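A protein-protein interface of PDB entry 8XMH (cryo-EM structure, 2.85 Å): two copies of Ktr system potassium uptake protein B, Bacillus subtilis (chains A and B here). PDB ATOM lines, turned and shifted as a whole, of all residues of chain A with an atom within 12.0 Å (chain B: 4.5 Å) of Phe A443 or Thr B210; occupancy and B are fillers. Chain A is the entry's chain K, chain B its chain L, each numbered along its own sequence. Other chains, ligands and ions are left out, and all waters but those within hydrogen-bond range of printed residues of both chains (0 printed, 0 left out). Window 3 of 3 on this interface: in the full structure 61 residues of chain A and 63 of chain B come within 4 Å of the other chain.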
ATOM      1  N   TYR A 329     -19.005 -11.362 -24.304  1.00  0.00           N
ATOM      2  CA  TYR A 329     -19.498 -10.157 -24.964  1.00  0.00           C
ATOM      3  C   TYR A 329     -18.942 -10.035 -26.378  1.00  0.00           C
ATOM      4  O   TYR A 329     -19.666  -9.654 -27.303  1.00  0.00           O
ATOM      5  CB  TYR A 329     -19.141  -8.922 -24.138  1.00  0.00           C
ATOM      6  CG  TYR A 329     -19.707  -7.634 -24.687  1.00  0.00           C
ATOM      7  CD1 TYR A 329     -20.988  -7.222 -24.357  1.00  0.00           C
ATOM      8  CD2 TYR A 329     -18.961  -6.828 -25.534  1.00  0.00           C
ATOM      9  CE1 TYR A 329     -21.511  -6.050 -24.859  1.00  0.00           C
ATOM     10  CE2 TYR A 329     -19.477  -5.657 -26.041  1.00  0.00           C
ATOM     11  CZ  TYR A 329     -20.750  -5.272 -25.699  1.00  0.00           C
ATOM     12  OH  TYR A 329     -21.265  -4.101 -26.202  1.00  0.00           O
ATOM     13  N   ASP A 439     -33.680   6.309 -17.367  1.00  0.00           N
ATOM     14  CA  ASP A 439     -32.475   5.869 -18.053  1.00  0.00           C
ATOM     15  C   ASP A 439     -31.863   7.001 -18.867  1.00  0.00           C
ATOM     16  O   ASP A 439     -32.570   7.796 -19.489  1.00  0.00           O
ATOM     17  CB  ASP A 439     -32.789   4.681 -18.958  1.00  0.00           C
ATOM     18  CG  ASP A 439     -33.339   3.496 -18.192  1.00  0.00           C
ATOM     19  OD1 ASP A 439     -33.400   3.570 -16.948  1.00  0.00           O
ATOM     20  OD2 ASP A 439     -33.714   2.491 -18.833  1.00  0.00           O
ATOM     21  N   GLY A 440     -30.543   7.075 -18.846  1.00  0.00           N
ATOM     22  CA  GLY A 440     -29.803   8.032 -19.656  1.00  0.00           C
ATOM     23  C   GLY A 440     -28.889   7.301 -20.617  1.00  0.00           C
ATOM     24  O   GLY A 440     -28.297   6.280 -20.263  1.00  0.00           O
ATOM     25  N   GLU A 441     -28.787   7.820 -21.836  1.00  0.00           N
ATOM     26  CA  GLU A 441     -27.970   7.214 -22.879  1.00  0.00           C
ATOM     27  C   GLU A 441     -26.632   7.936 -22.951  1.00  0.00           C
ATOM     28  O   GLU A 441     -26.584   9.147 -23.186  1.00  0.00           O
ATOM     29  CB  GLU A 441     -28.686   7.251 -24.230  1.00  0.00           C
ATOM     30  CG  GLU A 441     -29.451   8.534 -24.513  1.00  0.00           C
ATOM     31  CD  GLU A 441     -30.135   8.517 -25.868  1.00  0.00           C
ATOM     32  OE1 GLU A 441     -30.022   7.497 -26.580  1.00  0.00           O
ATOM     33  OE2 GLU A 441     -30.783   9.525 -26.220  1.00  0.00           O
ATOM     34  N   VAL A 442     -25.551   7.191 -22.737  1.00  0.00           N
ATOM     35  CA  VAL A 442     -24.193   7.713 -22.802  1.00  0.00           C
ATOM     36  C   VAL A 442     -23.371   6.774 -23.674  1.00  0.00           C
ATOM     37  O   VAL A 442     -23.425   5.552 -23.499  1.00  0.00           O
ATOM     38  CB  VAL A 442     -23.576   7.869 -21.397  1.00  0.00           C
ATOM     39  CG1 VAL A 442     -23.924   6.679 -20.521  1.00  0.00           C
ATOM     40  CG2 VAL A 442     -22.074   8.052 -21.478  1.00  0.00           C
ATOM     41  N   PHE A 443     -22.639   7.338 -24.631  1.00  0.00           N
ATOM     42  CA  PHE A 443     -21.869   6.551 -25.585  1.00  0.00           C
ATOM     43  C   PHE A 443     -20.518   6.201 -24.972  1.00  0.00           C
ATOM     44  O   PHE A 443     -19.705   7.091 -24.698  1.00  0.00           O
ATOM     45  CB  PHE A 443     -21.685   7.317 -26.896  1.00  0.00           C
ATOM     46  CG  PHE A 443     -22.948   7.947 -27.415  1.00  0.00           C
ATOM     47  CD1 PHE A 443     -24.156   7.269 -27.370  1.00  0.00           C
ATOM     48  CD2 PHE A 443     -22.925   9.225 -27.945  1.00  0.00           C
ATOM     49  CE1 PHE A 443     -25.310   7.855 -27.837  1.00  0.00           C
ATOM     50  CE2 PHE A 443     -24.076   9.814 -28.416  1.00  0.00           C
ATOM     51  CZ  PHE A 443     -25.269   9.128 -28.364  1.00  0.00           C
ATOM     52  N   THR A 444     -20.278   4.910 -24.763  1.00  0.00           N
ATOM     53  CA  THR A 444     -19.069   4.419 -24.113  1.00  0.00           C
ATOM     54  C   THR A 444     -18.227   3.595 -25.077  1.00  0.00           C
ATOM     55  O   THR A 444     -17.678   2.551 -24.716  1.00  0.00           O
ATOM     56  CB  THR A 444     -19.408   3.599 -22.871  1.00  0.00           C
ATOM     57  OG1 THR A 444     -20.270   2.515 -23.233  1.00  0.00           O
ATOM     58  CG2 THR A 444     -20.105   4.462 -21.836  1.00  0.00           C
ATOM     59  N   GLY A 445     -18.111   4.055 -26.316  1.00  0.00           N
ATOM     60  CA  GLY A 445     -17.317   3.359 -27.308  1.00  0.00           C
ATOM     61  C   GLY A 445     -15.829   3.622 -27.181  1.00  0.00           C
ATOM     62  O   GLY A 445     -15.302   3.730 -26.075  1.00  0.00           O
ATOM     63  N   GLN B 120     -22.666   4.884 -32.988  1.00  0.00           N
ATOM     64  CA  GLN B 120     -24.003   5.336 -32.646  1.00  0.00           C
ATOM     65  C   GLN B 120     -24.882   4.155 -32.244  1.00  0.00           C
ATOM     66  O   GLN B 120     -24.704   3.041 -32.746  1.00  0.00           O
ATOM     67  CB  GLN B 120     -24.633   6.065 -33.829  1.00  0.00           C
ATOM     68  CG  GLN B 120     -25.188   7.436 -33.488  1.00  0.00           C
ATOM     69  CD  GLN B 120     -24.126   8.385 -32.972  1.00  0.00           C
ATOM     70  OE1 GLN B 120     -22.982   8.364 -33.425  1.00  0.00           O
ATOM     71  NE2 GLN B 120     -24.500   9.224 -32.015  1.00  0.00           N
ATOM     72  N   PRO B 121     -25.836   4.363 -31.331  1.00  0.00           N
ATOM     73  CA  PRO B 121     -26.751   3.270 -30.973  1.00  0.00           C
ATOM     74  C   PRO B 121     -27.909   3.099 -31.938  1.00  0.00           C
ATOM     75  O   PRO B 121     -28.447   1.987 -32.034  1.00  0.00           O
ATOM     76  CB  PRO B 121     -27.252   3.678 -29.583  1.00  0.00           C
ATOM     77  CG  PRO B 121     -27.203   5.167 -29.610  1.00  0.00           C
ATOM     78  CD  PRO B 121     -26.016   5.538 -30.462  1.00  0.00           C
ATOM     79  N   LEU B 129     -25.758  13.860 -39.515  1.00  0.00           N
ATOM     80  CA  LEU B 129     -24.635  14.167 -38.636  1.00  0.00           C
ATOM     81  C   LEU B 129     -23.331  14.265 -39.419  1.00  0.00           C
ATOM     82  O   LEU B 129     -22.468  15.090 -39.095  1.00  0.00           O
ATOM     83  CB  LEU B 129     -24.529  13.110 -37.537  1.00  0.00           C
ATOM     84  CG  LEU B 129     -23.404  13.251 -36.511  1.00  0.00           C
ATOM     85  CD1 LEU B 129     -23.544  14.546 -35.729  1.00  0.00           C
ATOM     86  CD2 LEU B 129     -23.393  12.055 -35.574  1.00  0.00           C
ATOM     87  N   GLY B 208     -15.908  15.419 -29.363  1.00  0.00           N
ATOM     88  CA  GLY B 208     -16.965  14.592 -29.906  1.00  0.00           C
ATOM     89  C   GLY B 208     -17.807  15.320 -30.929  1.00  0.00           C
ATOM     90  O   GLY B 208     -18.176  16.479 -30.729  1.00  0.00           O
ATOM     91  N   PHE B 209     -18.103  14.651 -32.043  1.00  0.00           N
ATOM     92  CA  PHE B 209     -18.959  15.252 -33.059  1.00  0.00           C
ATOM     93  C   PHE B 209     -20.402  15.345 -32.582  1.00  0.00           C
ATOM     94  O   PHE B 209     -21.112  16.292 -32.931  1.00  0.00           O
ATOM     95  CB  PHE B 209     -18.865  14.452 -34.357  1.00  0.00           C
ATOM     96  CG  PHE B 209     -17.478  14.394 -34.930  1.00  0.00           C
ATOM     97  CD1 PHE B 209     -16.676  15.523 -34.947  1.00  0.00           C
ATOM     98  CD2 PHE B 209     -16.972  13.210 -35.440  1.00  0.00           C
ATOM     99  CE1 PHE B 209     -15.398  15.474 -35.470  1.00  0.00           C
ATOM    100  CE2 PHE B 209     -15.694  13.154 -35.966  1.00  0.00           C
ATOM    101  CZ  PHE B 209     -14.907  14.288 -35.980  1.00  0.00           C
ATOM    102  N   THR B 210     -20.849  14.372 -31.788  1.00  0.00           N
ATOM    103  CA  THR B 210     -22.195  14.428 -31.228  1.00  0.00           C
ATOM    104  C   THR B 210     -22.308  15.531 -30.182  1.00  0.00           C
ATOM    105  O   THR B 210     -23.360  16.167 -30.054  1.00  0.00           O
ATOM    106  CB  THR B 210     -22.567  13.071 -30.631  1.00  0.00           C
ATOM    107  OG1 THR B 210     -22.232  12.035 -31.563  1.00  0.00           O
ATOM    108  CG2 THR B 210     -24.057  13.000 -30.344  1.00  0.00           C
ATOM    109  N   VAL B 211     -21.236  15.767 -29.423  1.00  0.00           N
ATOM    110  CA  VAL B 211     -21.232  16.847 -28.440  1.00  0.00           C
ATOM    111  C   VAL B 211     -21.295  18.202 -29.131  1.00  0.00           C
ATOM    112  O   VAL B 211     -22.020  19.101 -28.692  1.00  0.00           O
ATOM    113  CB  VAL B 211     -19.996  16.727 -27.529  1.00  0.00           C
ATOM    114  CG1 VAL B 211     -19.921  17.893 -26.561  1.00  0.00           C
ATOM    115  CG2 VAL B 211     -20.028  15.414 -26.773  1.00  0.00           C
ATOM    116  N   LEU B 212     -20.538  18.374 -30.218  1.00  0.00           N
ATOM    117  CA  LEU B 212     -20.550  19.641 -30.945  1.00  0.00           C
ATOM    118  C   LEU B 212     -21.908  19.905 -31.581  1.00  0.00           C
ATOM    119  O   LEU B 212     -22.388  21.043 -31.585  1.00  0.00           O
ATOM    120  CB  LEU B 212     -19.456  19.647 -32.009  1.00  0.00           C
ATOM    121  CG  LEU B 212     -18.014  19.746 -31.517  1.00  0.00           C
ATOM    122  CD1 LEU B 212     -17.046  19.568 -32.672  1.00  0.00           C
ATOM    123  CD2 LEU B 212     -17.785  21.076 -30.826  1.00  0.00           C
ATOM    124  N   PHE B 213     -22.538  18.863 -32.128  1.00  0.00           N
ATOM    125  CA  PHE B 213     -23.852  19.017 -32.741  1.00  0.00           C
ATOM    126  C   PHE B 213     -24.913  19.388 -31.713  1.00  0.00           C
ATOM    127  O   PHE B 213     -25.876  20.086 -32.044  1.00  0.00           O
ATOM    128  CB  PHE B 213     -24.234  17.728 -33.470  1.00  0.00           C
ATOM    129  CG  PHE B 213     -25.577  17.776 -34.139  1.00  0.00           C
ATOM    130  CD1 PHE B 213     -25.740  18.429 -35.350  1.00  0.00           C
ATOM    131  CD2 PHE B 213     -26.675  17.151 -33.569  1.00  0.00           C
ATOM    132  CE1 PHE B 213     -26.972  18.471 -35.970  1.00  0.00           C
ATOM    133  CE2 PHE B 213     -27.910  17.189 -34.184  1.00  0.00           C
ATOM    134  CZ  PHE B 213     -28.058  17.850 -35.387  1.00  0.00           C
ATOM    135  N   ASP B 214     -24.757  18.929 -30.470  1.00  0.00           N
ATOM    136  CA  ASP B 214     -25.727  19.257 -29.430  1.00  0.00           C
ATOM    137  C   ASP B 214     -25.588  20.705 -28.974  1.00  0.00           C
ATOM    138  O   ASP B 214     -26.589  21.367 -28.686  1.00  0.00           O
ATOM    139  CB  ASP B 214     -25.561  18.301 -28.251  1.00  0.00           C
ATOM    140  CG  ASP B 214     -26.775  18.273 -27.348  1.00  0.00           C
ATOM    141  OD1 ASP B 214     -27.795  18.901 -27.697  1.00  0.00           O
ATOM    142  OD2 ASP B 214     -26.709  17.617 -26.289  1.00  0.00           O
ATOM    143  N   HIS B 227     -24.716  12.523 -22.332  1.00  0.00           N
ATOM    144  CA  HIS B 227     -23.381  12.397 -22.904  1.00  0.00           C
ATOM    145  C   HIS B 227     -22.714  13.756 -23.071  1.00  0.00           C
ATOM    146  O   HIS B 227     -21.513  13.895 -22.822  1.00  0.00           O
ATOM    147  CB  HIS B 227     -23.453  11.669 -24.244  1.00  0.00           C
ATOM    148  CG  HIS B 227     -22.119  11.456 -24.887  1.00  0.00           C
ATOM    149  ND1 HIS B 227     -21.355  10.332 -24.661  1.00  0.00           N
ATOM    150  CD2 HIS B 227     -21.411  12.225 -25.747  1.00  0.00           C
ATOM    151  CE1 HIS B 227     -20.235  10.417 -25.355  1.00  0.00           C
ATOM    152  NE2 HIS B 227     -20.243  11.557 -26.022  1.00  0.00           N
ATOM    153  N   SER B 307     -16.633   9.845 -27.857  1.00  0.00           N
ATOM    154  CA  SER B 307     -16.835   8.550 -28.497  1.00  0.00           C
ATOM    155  C   SER B 307     -16.726   8.656 -30.013  1.00  0.00           C
ATOM    156  O   SER B 307     -16.134   7.786 -30.661  1.00  0.00           O
ATOM    157  CB  SER B 307     -18.189   7.973 -28.091  1.00  0.00           C
ATOM    158  OG  SER B 307     -18.371   6.676 -28.632  1.00  0.00           O
ATOM    159  N   ALA B 308     -17.287   9.710 -30.596  1.00  0.00           N
ATOM    160  CA  ALA B 308     -17.215   9.957 -32.034  1.00  0.00           C
ATOM    161  C   ALA B 308     -16.436  11.253 -32.224  1.00  0.00           C
ATOM    162  O   ALA B 308     -17.019  12.334 -32.318  1.00  0.00           O
ATOM    163  CB  ALA B 308     -18.604  10.034 -32.656  1.00  0.00           C
ATOM    164  N   THR B 317     -16.038   9.171 -21.355  1.00  0.00           N
ATOM    165  CA  THR B 317     -17.295   8.642 -20.839  1.00  0.00           C
ATOM    166  C   THR B 317     -17.165   7.194 -20.389  1.00  0.00           C
ATOM    167  O   THR B 317     -17.867   6.774 -19.466  1.00  0.00           O
ATOM    168  CB  THR B 317     -18.394   8.768 -21.891  1.00  0.00           C
ATOM    169  OG1 THR B 317     -17.950   8.180 -23.119  1.00  0.00           O
ATOM    170  CG2 THR B 317     -18.740  10.227 -22.121  1.00  0.00           C
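Hydrophobic or aromatic side chains of chain A within 4 Å of the printed part of chain B: Val A442 and Phe A443. Of the 14 printed residues of chain B, 6 touch a printed residue of chain A. Among the printed residues, no Asp or Glu carboxylate lies within 4 Å of a Lys or Arg side-chain nitrogen of the other chain.
Tyr A329 touches none of the printed residues of chain B. Of the printed residues of chain B, Phe A443 touches Gln B120, Pro B121, Thr B210, His B227, Ser B307 and Thr B317. Printed residues of chain B within 4 Å of Thr A444: Thr B317 (3.996 Å). Of chain A, only Phe A443 comes within 4 Å of Pro B121. Leu B129 touches none of the printed residues of chain A. No residue of chain A comes within 4 Å of Gly B208. No residue of chain A comes within 4 Å of Phe B209. Of chain A, only Phe A443 (3.7 Å) comes within 4 Å of Thr B210. No residue of chain A comes within 4 Å of Val B211. No residue of chain A comes within 4 Å of Leu B212. No residue of chain A comes within 4 Å of Phe B213. No residue of chain A comes within 4 Å of Asp B214. Ser B307 touches just these residues of chain A: Phe A443 (3.8 Å) and Gly A445 (3.5 Å). No residue of chain A comes within 4 Å of Ala B308. Printed residues of chain A within 4 Å of Thr B317: Val A442, Phe A443 and Thr A444. The nearest residue of chain A that does not touch Thr B210 is Glu A441 (8.5 Å).
His B227 touches Glu A441. ND1 of His B227 touches CG2 of Val A442 (3.98 Å). Thr B317 touches Val A442 (CB to CG2, 3.8 Å). Gln B120 touches Phe A443 (NE2 to CE2, 3.7 Å). Pro B121 touches Phe A443 (CD to CE1, 3.6 Å). Thr B210 touches Phe A443. Ser B307 touches Phe A443 (CB to CB, 3.8 Å). Thr A444 touches Thr B317 (CG2 to O, 3.996 Å). OG of Ser B307 touches N of Gly A445, at 3.5 Å.
No position is printed for both chains. Of the 11 pairs that touch across the chains among the printed residues, none has its exchanged pair printed and touching as well.
A ring nitrogen (ND1) of His B227 lies within hydrogen-bond range of the backbone NH of Phe A443, at 3.3 Å. O of Phe A443 lies within hydrogen-bond range of OG1 of Thr B317 (2.6 Å).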
